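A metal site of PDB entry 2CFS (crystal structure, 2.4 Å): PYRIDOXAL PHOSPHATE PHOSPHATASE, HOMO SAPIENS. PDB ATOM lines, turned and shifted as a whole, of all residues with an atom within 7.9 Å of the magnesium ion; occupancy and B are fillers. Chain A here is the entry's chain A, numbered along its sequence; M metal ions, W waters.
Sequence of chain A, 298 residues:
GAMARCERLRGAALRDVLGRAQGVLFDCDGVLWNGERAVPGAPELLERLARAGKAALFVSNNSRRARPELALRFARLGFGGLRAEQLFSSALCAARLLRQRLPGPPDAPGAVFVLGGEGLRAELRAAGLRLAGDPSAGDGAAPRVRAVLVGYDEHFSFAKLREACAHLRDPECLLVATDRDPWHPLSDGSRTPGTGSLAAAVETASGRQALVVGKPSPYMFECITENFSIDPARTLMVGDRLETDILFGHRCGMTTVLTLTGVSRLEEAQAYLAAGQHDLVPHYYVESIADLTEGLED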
ATOM      1  N   PHE A  26      18.190  15.889  -2.943  1.00  0.00           N
ATOM      2  CA  PHE A  26      16.791  15.968  -3.350  1.00  0.00           C
ATOM      3  C   PHE A  26      16.295  17.399  -3.450  1.00  0.00           C
ATOM      4  O   PHE A  26      16.519  18.208  -2.534  1.00  0.00           O
ATOM      5  CB  PHE A  26      15.848  15.270  -2.372  1.00  0.00           C
ATOM      6  CG  PHE A  26      16.044  13.803  -2.285  1.00  0.00           C
ATOM      7  CD1 PHE A  26      15.311  12.930  -3.113  1.00  0.00           C
ATOM      8  CD2 PHE A  26      16.923  13.262  -1.351  1.00  0.00           C
ATOM      9  CE1 PHE A  26      15.476  11.538  -3.004  1.00  0.00           C
ATOM     10  CE2 PHE A  26      17.094  11.906  -1.247  1.00  0.00           C
ATOM     11  CZ  PHE A  26      16.385  11.040  -2.059  1.00  0.00           C
ATOM     12  N   ASP A  27      15.633  17.672  -4.564  1.00  0.00           N
ATOM     13  CA  ASP A  27      14.687  18.768  -4.674  1.00  0.00           C
ATOM     14  C   ASP A  27      13.447  18.357  -3.860  1.00  0.00           C
ATOM     15  O   ASP A  27      13.258  17.155  -3.573  1.00  0.00           O
ATOM     16  CB  ASP A  27      14.298  18.931  -6.150  1.00  0.00           C
ATOM     17  CG  ASP A  27      13.173  19.889  -6.326  1.00  0.00           C
ATOM     18  OD1 ASP A  27      13.201  20.963  -5.717  1.00  0.00           O
ATOM     19  OD2 ASP A  27      12.219  19.575  -7.032  1.00  0.00           O
ATOM     20  N   CYS A  28      12.586  19.322  -3.521  1.00  0.00           N
ATOM     21  CA  CYS A  28      11.425  19.027  -2.685  1.00  0.00           C
ATOM     22  C   CYS A  28      10.038  18.927  -3.405  1.00  0.00           C
ATOM     23  O   CYS A  28       9.463  17.837  -3.540  1.00  0.00           O
ATOM     24  CB  CYS A  28      11.407  19.997  -1.468  1.00  0.00           C
ATOM     25  SG  CYS A  28      13.007  19.980  -0.490  1.00  0.00           S
ATOM     26  N   ASP A  29       9.506  20.046  -3.854  1.00  0.00           N
ATOM     27  CA  ASP A  29       8.173  20.048  -4.445  1.00  0.00           C
ATOM     28  C   ASP A  29       8.218  19.387  -5.792  1.00  0.00           C
ATOM     29  O   ASP A  29       9.137  19.569  -6.559  1.00  0.00           O
ATOM     30  CB  ASP A  29       7.521  21.441  -4.525  1.00  0.00           C
ATOM     31  CG  ASP A  29       6.035  21.379  -4.866  1.00  0.00           C
ATOM     32  OD1 ASP A  29       5.181  21.382  -3.936  1.00  0.00           O
ATOM     33  OD2 ASP A  29       5.708  21.274  -6.076  1.00  0.00           O
ATOM     34  N   GLY A  30       7.239  18.536  -6.033  1.00  0.00           N
ATOM     35  CA  GLY A  30       7.243  17.645  -7.195  1.00  0.00           C
ATOM     36  C   GLY A  30       8.094  16.392  -7.054  1.00  0.00           C
ATOM     37  O   GLY A  30       8.221  15.626  -8.000  1.00  0.00           O
ATOM     38  N   VAL A  31       8.712  16.203  -5.885  1.00  0.00           N
ATOM     39  CA  VAL A  31       9.643  15.116  -5.660  1.00  0.00           C
ATOM     40  C   VAL A  31       9.309  14.353  -4.390  1.00  0.00           C
ATOM     41  O   VAL A  31       9.062  13.142  -4.440  1.00  0.00           O
ATOM     42  CB  VAL A  31      11.123  15.606  -5.597  1.00  0.00           C
ATOM     43  CG1 VAL A  31      12.068  14.426  -5.297  1.00  0.00           C
ATOM     44  CG2 VAL A  31      11.507  16.275  -6.903  1.00  0.00           C
ATOM     45  N   LEU A  32       9.252  15.052  -3.256  1.00  0.00           N
ATOM     46  CA  LEU A  32       8.900  14.457  -1.964  1.00  0.00           C
ATOM     47  C   LEU A  32       7.420  14.555  -1.743  1.00  0.00           C
ATOM     48  O   LEU A  32       6.836  13.721  -1.041  1.00  0.00           O
ATOM     49  CB  LEU A  32       9.636  15.189  -0.821  1.00  0.00           C
ATOM     50  CG  LEU A  32      11.148  15.289  -0.885  1.00  0.00           C
ATOM     51  CD1 LEU A  32      11.656  16.152   0.253  1.00  0.00           C
ATOM     52  CD2 LEU A  32      11.771  13.899  -0.841  1.00  0.00           C
ATOM     53  N   TRP A  33       6.826  15.582  -2.355  1.00  0.00           N
ATOM     54  CA  TRP A  33       5.421  15.930  -2.172  1.00  0.00           C
ATOM     55  C   TRP A  33       4.913  16.809  -3.345  1.00  0.00           C
ATOM     56  O   TRP A  33       5.719  17.322  -4.132  1.00  0.00           O
ATOM     57  CB  TRP A  33       5.237  16.662  -0.821  1.00  0.00           C
ATOM     58  CG  TRP A  33       6.179  17.819  -0.593  1.00  0.00           C
ATOM     59  CD1 TRP A  33       6.222  18.995  -1.293  1.00  0.00           C
ATOM     60  CD2 TRP A  33       7.193  17.936   0.438  1.00  0.00           C
ATOM     61  NE1 TRP A  33       7.201  19.811  -0.799  1.00  0.00           N
ATOM     62  CE2 TRP A  33       7.798  19.204   0.276  1.00  0.00           C
ATOM     63  CE3 TRP A  33       7.638  17.103   1.491  1.00  0.00           C
ATOM     64  CZ2 TRP A  33       8.866  19.672   1.123  1.00  0.00           C
ATOM     65  CZ3 TRP A  33       8.687  17.570   2.343  1.00  0.00           C
ATOM     66  CH2 TRP A  33       9.282  18.841   2.140  1.00  0.00           C
ATOM     67  N   ASN A  34       3.589  16.930  -3.459  1.00  0.00           N
ATOM     68  CA  ASN A  34       2.916  17.984  -4.224  1.00  0.00           C
ATOM     69  C   ASN A  34       1.839  18.607  -3.341  1.00  0.00           C
ATOM     70  O   ASN A  34       0.854  17.917  -2.980  1.00  0.00           O
ATOM     71  CB  ASN A  34       2.274  17.433  -5.482  1.00  0.00           C
ATOM     72  CG  ASN A  34       3.284  16.834  -6.427  1.00  0.00           C
ATOM     73  OD1 ASN A  34       3.321  15.619  -6.627  1.00  0.00           O
ATOM     74  ND2 ASN A  34       4.127  17.681  -6.986  1.00  0.00           N
ATOM     75  N   VAL A  59      17.716  20.479  -1.506  1.00  0.00           N
ATOM     76  CA  VAL A  59      18.081  21.702  -2.220  1.00  0.00           C
ATOM     77  C   VAL A  59      16.818  22.276  -2.853  1.00  0.00           C
ATOM     78  O   VAL A  59      16.213  21.673  -3.745  1.00  0.00           O
ATOM     79  CB  VAL A  59      19.305  21.487  -3.180  1.00  0.00           C
ATOM     80  CG1 VAL A  59      19.005  20.416  -4.205  1.00  0.00           C
ATOM     81  CG2 VAL A  59      19.731  22.785  -3.836  1.00  0.00           C
ATOM     82  N   SER A  60      16.388  23.428  -2.323  1.00  0.00           N
ATOM     83  CA  SER A  60      15.144  24.096  -2.710  1.00  0.00           C
ATOM     84  C   SER A  60      15.365  25.541  -3.178  1.00  0.00           C
ATOM     85  O   SER A  60      16.168  26.298  -2.619  1.00  0.00           O
ATOM     86  CB  SER A  60      14.197  24.066  -1.527  1.00  0.00           C
ATOM     87  OG  SER A  60      13.002  24.745  -1.786  1.00  0.00           O
ATOM     88  N   ASN A  61      14.613  25.934  -4.193  1.00  0.00           N
ATOM     89  CA  ASN A  61      14.625  27.308  -4.698  1.00  0.00           C
ATOM     90  C   ASN A  61      13.635  28.201  -3.963  1.00  0.00           C
ATOM     91  O   ASN A  61      13.436  29.344  -4.345  1.00  0.00           O
ATOM     92  CB  ASN A  61      14.360  27.326  -6.218  1.00  0.00           C
ATOM     93  CG  ASN A  61      15.609  27.137  -7.020  1.00  0.00           C
ATOM     94  OD1 ASN A  61      16.718  27.186  -6.487  1.00  0.00           O
ATOM     95  ND2 ASN A  61      15.445  26.929  -8.316  1.00  0.00           N
ATOM     96  N   ASP A 181      12.991  30.572 -11.388  1.00  0.00           N
ATOM     97  CA  ASP A 181      11.794  29.759 -11.623  1.00  0.00           C
ATOM     98  C   ASP A 181      10.688  30.659 -12.175  1.00  0.00           C
ATOM     99  O   ASP A 181      10.337  31.654 -11.540  1.00  0.00           O
ATOM    100  CB  ASP A 181      11.324  29.005 -10.363  1.00  0.00           C
ATOM    101  CG  ASP A 181      12.272  27.903  -9.932  1.00  0.00           C
ATOM    102  OD1 ASP A 181      12.058  27.350  -8.831  1.00  0.00           O
ATOM    103  OD2 ASP A 181      13.232  27.576 -10.649  1.00  0.00           O
ATOM    104  N   HIS A 184       5.058  28.268 -10.843  1.00  0.00           N
ATOM    105  CA  HIS A 184       4.921  27.147  -9.911  1.00  0.00           C
ATOM    106  C   HIS A 184       3.496  26.584  -9.936  1.00  0.00           C
ATOM    107  O   HIS A 184       2.518  27.327  -9.773  1.00  0.00           O
ATOM    108  CB  HIS A 184       5.306  27.578  -8.471  1.00  0.00           C
ATOM    109  CG  HIS A 184       6.745  27.989  -8.348  1.00  0.00           C
ATOM    110  ND1 HIS A 184       7.782  27.078  -8.314  1.00  0.00           N
ATOM    111  CD2 HIS A 184       7.319  29.218  -8.301  1.00  0.00           C
ATOM    112  CE1 HIS A 184       8.936  27.720  -8.231  1.00  0.00           C
ATOM    113  NE2 HIS A 184       8.681  29.024  -8.225  1.00  0.00           N
ATOM    114  N   PRO A 185       3.380  25.259 -10.124  1.00  0.00           N
ATOM    115  CA  PRO A 185       2.076  24.601 -10.195  1.00  0.00           C
ATOM    116  C   PRO A 185       1.399  24.565  -8.829  1.00  0.00           C
ATOM    117  O   PRO A 185       2.058  24.337  -7.805  1.00  0.00           O
ATOM    118  CB  PRO A 185       2.436  23.176 -10.669  1.00  0.00           C
ATOM    119  CG  PRO A 185       3.834  22.967 -10.179  1.00  0.00           C
ATOM    120  CD  PRO A 185       4.507  24.319 -10.239  1.00  0.00           C
ATOM    121  N   LYS A 215      19.365  26.756  -7.994  1.00  0.00           N
ATOM    122  CA  LYS A 215      19.493  25.892  -9.146  1.00  0.00           C
ATOM    123  C   LYS A 215      18.856  26.604 -10.355  1.00  0.00           C
ATOM    124  O   LYS A 215      17.792  27.223 -10.206  1.00  0.00           O
ATOM    125  CB  LYS A 215      18.725  24.585  -8.898  1.00  0.00           C
ATOM    126  CG  LYS A 215      19.061  23.829  -7.628  1.00  0.00           C
ATOM    127  CD  LYS A 215      17.995  22.794  -7.332  1.00  0.00           C
ATOM    128  CE  LYS A 215      16.817  23.381  -6.625  1.00  0.00           C
ATOM    129  NZ  LYS A 215      15.668  22.432  -6.571  1.00  0.00           N
ATOM    130  N   VAL A 238      18.300  14.372  -7.553  1.00  0.00           N
ATOM    131  CA  VAL A 238      16.954  13.944  -7.861  1.00  0.00           C
ATOM    132  C   VAL A 238      16.014  15.169  -7.859  1.00  0.00           C
ATOM    133  O   VAL A 238      15.904  15.873  -6.865  1.00  0.00           O
ATOM    134  CB  VAL A 238      16.462  12.845  -6.849  1.00  0.00           C
ATOM    135  CG1 VAL A 238      15.046  12.355  -7.212  1.00  0.00           C
ATOM    136  CG2 VAL A 238      17.473  11.653  -6.799  1.00  0.00           C
ATOM    137  N   GLY A 239      15.348  15.409  -8.997  1.00  0.00           N
ATOM    138  CA  GLY A 239      14.460  16.553  -9.197  1.00  0.00           C
ATOM    139  C   GLY A 239      13.387  16.262 -10.230  1.00  0.00           C
ATOM    140  O   GLY A 239      13.427  15.218 -10.890  1.00  0.00           O
ATOM    141  N   ASP A 240      12.425  17.162 -10.386  1.00  0.00           N
ATOM    142  CA  ASP A 240      11.287  16.957 -11.270  1.00  0.00           C
ATOM    143  C   ASP A 240      11.272  17.921 -12.466  1.00  0.00           C
ATOM    144  O   ASP A 240      10.338  17.907 -13.294  1.00  0.00           O
ATOM    145  CB  ASP A 240       9.967  17.147 -10.509  1.00  0.00           C
ATOM    146  CG  ASP A 240       9.757  18.579 -10.093  1.00  0.00           C
ATOM    147  OD1 ASP A 240      10.623  19.102  -9.389  1.00  0.00           O
ATOM    148  OD2 ASP A 240       8.726  19.175 -10.429  1.00  0.00           O
ATOM    149  N   ARG A 241      12.302  18.760 -12.539  1.00  0.00           N
ATOM    150  CA  ARG A 241      12.266  19.908 -13.412  1.00  0.00           C
ATOM    151  C   ARG A 241      13.598  19.984 -14.121  1.00  0.00           C
ATOM    152  O   ARG A 241      14.618  20.281 -13.491  1.00  0.00           O
ATOM    153  CB  ARG A 241      11.957  21.176 -12.593  1.00  0.00           C
ATOM    154  CG  ARG A 241      11.458  22.317 -13.421  1.00  0.00           C
ATOM    155  CD  ARG A 241      10.735  23.378 -12.595  1.00  0.00           C
ATOM    156  NE  ARG A 241      10.130  24.377 -13.484  1.00  0.00           N
ATOM    157  CZ  ARG A 241       9.276  25.326 -13.120  1.00  0.00           C
ATOM    158  NH1 ARG A 241       8.850  25.437 -11.866  1.00  0.00           N
ATOM    159  NH2 ARG A 241       8.808  26.159 -14.051  1.00  0.00           N
ATOM    160  N   THR A 244      16.120  23.048 -14.293  1.00  0.00           N
ATOM    161  CA  THR A 244      16.504  23.483 -12.948  1.00  0.00           C
ATOM    162  C   THR A 244      17.350  22.416 -12.240  1.00  0.00           C
ATOM    163  O   THR A 244      18.557  22.572 -12.049  1.00  0.00           O
ATOM    164  CB  THR A 244      15.234  23.772 -12.160  1.00  0.00           C
ATOM    165  OG1 THR A 244      14.654  24.941 -12.710  1.00  0.00           O
ATOM    166  CG2 THR A 244      15.501  23.994 -10.683  1.00  0.00           C
ATOM    167  N   ASP A 245      16.678  21.313 -11.915  1.00  0.00           N
ATOM    168  CA  ASP A 245      17.246  20.193 -11.182  1.00  0.00           C
ATOM    169  C   ASP A 245      18.181  19.374 -12.035  1.00  0.00           C
ATOM    170  O   ASP A 245      19.272  19.032 -11.580  1.00  0.00           O
ATOM    171  CB  ASP A 245      16.122  19.302 -10.603  1.00  0.00           C
ATOM    172  CG  ASP A 245      15.122  20.084  -9.773  1.00  0.00           C
ATOM    173  OD1 ASP A 245      15.568  20.890  -8.919  1.00  0.00           O
ATOM    174  OD2 ASP A 245      13.909  19.931  -9.992  1.00  0.00           O
ATOM    175  N   THR A 259      12.308  12.487 -11.652  1.00  0.00           N
ATOM    176  CA  THR A 259      11.107  11.882 -11.129  1.00  0.00           C
ATOM    177  C   THR A 259       9.916  12.501 -11.877  1.00  0.00           C
ATOM    178  O   THR A 259       9.955  13.682 -12.239  1.00  0.00           O
ATOM    179  CB  THR A 259      11.045  11.996  -9.598  1.00  0.00           C
ATOM    180  OG1 THR A 259       9.975  11.188  -9.111  1.00  0.00           O
ATOM    181  CG2 THR A 259      10.832  13.424  -9.151  1.00  0.00           C
ATOM    182  N   GLY A 262       6.323  15.496 -10.828  1.00  0.00           N
ATOM    183  CA  GLY A 262       6.270  16.966 -10.876  1.00  0.00           C
ATOM    184  C   GLY A 262       6.097  17.619 -12.232  1.00  0.00           C
ATOM    185  O   GLY A 262       5.237  17.224 -13.005  1.00  0.00           O
ATOM    186  N   VAL A 263       6.914  18.638 -12.498  1.00  0.00           N
ATOM    187  CA  VAL A 263       6.762  19.546 -13.638  1.00  0.00           C
ATOM    188  C   VAL A 263       7.066  18.915 -15.014  1.00  0.00           C
ATOM    189  O   VAL A 263       6.239  18.994 -15.925  1.00  0.00           O
ATOM    190  CB  VAL A 263       7.618  20.860 -13.461  1.00  0.00           C
ATOM    191  CG1 VAL A 263       7.518  21.791 -14.720  1.00  0.00           C
ATOM    192  CG2 VAL A 263       7.230  21.598 -12.185  1.00  0.00           C
HETATM  193 MG    MG M   1      10.676  20.605  -7.867  1.00  0.00          MG
HETATM  194  O   HOH W   1      10.754  22.218  -6.823  1.00  0.00           O
HETATM  195  O   HOH W   2      12.036  21.503  -9.109  1.00  0.00           O
HETATM  196  O   HOH W   3       9.048  21.303  -8.962  1.00  0.00           O
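The side-chain carboxylate of Asp 240 sits at hydrogen-bond distance from the backbone NH of Val 263 (2.8 Å). NZ of Lys 215 is in salt-bridge range of OD1 of Asp 245. The backbone NH of Asp 27 lies within hydrogen-bond range of the backbone carbonyl oxygen of Val 238. NZ of Lys 215 lies within salt-bridge range of OD1 of Asp 27 (3.0 Å). The backbone NH (N) of Asp 240 sits at hydrogen-bond distance from the side-chain carboxylate (OD2) of Asp 245. The side-chain carboxylate (OD2) of Asp 245 sits at hydrogen-bond distance from the backbone NH (N) of Arg 241 (3.2 Å).
Residues that only touch the magnesium ion: Asp 245 (3.9 Å). Within 4 Å of the magnesium ion: Asp 27, Asp 29, Asp 240 and Asp 245. Along chain A the residues within 4 Å of the magnesium ion span positions 27 to 245.
Water W1 binds the magnesium ion, at 1.9 Å. OD2 of Asp 27 is bound to the magnesium ion, at 2.0 Å. Water W2 is bound to the magnesium ion (2.0 Å). Water W3 binds the magnesium ion (2.1 Å). OD1 of Asp 240 is bound to the magnesium ion (2.1 Å). The backbone carbonyl oxygen (O) of Asp 29 binds the magnesium ion.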
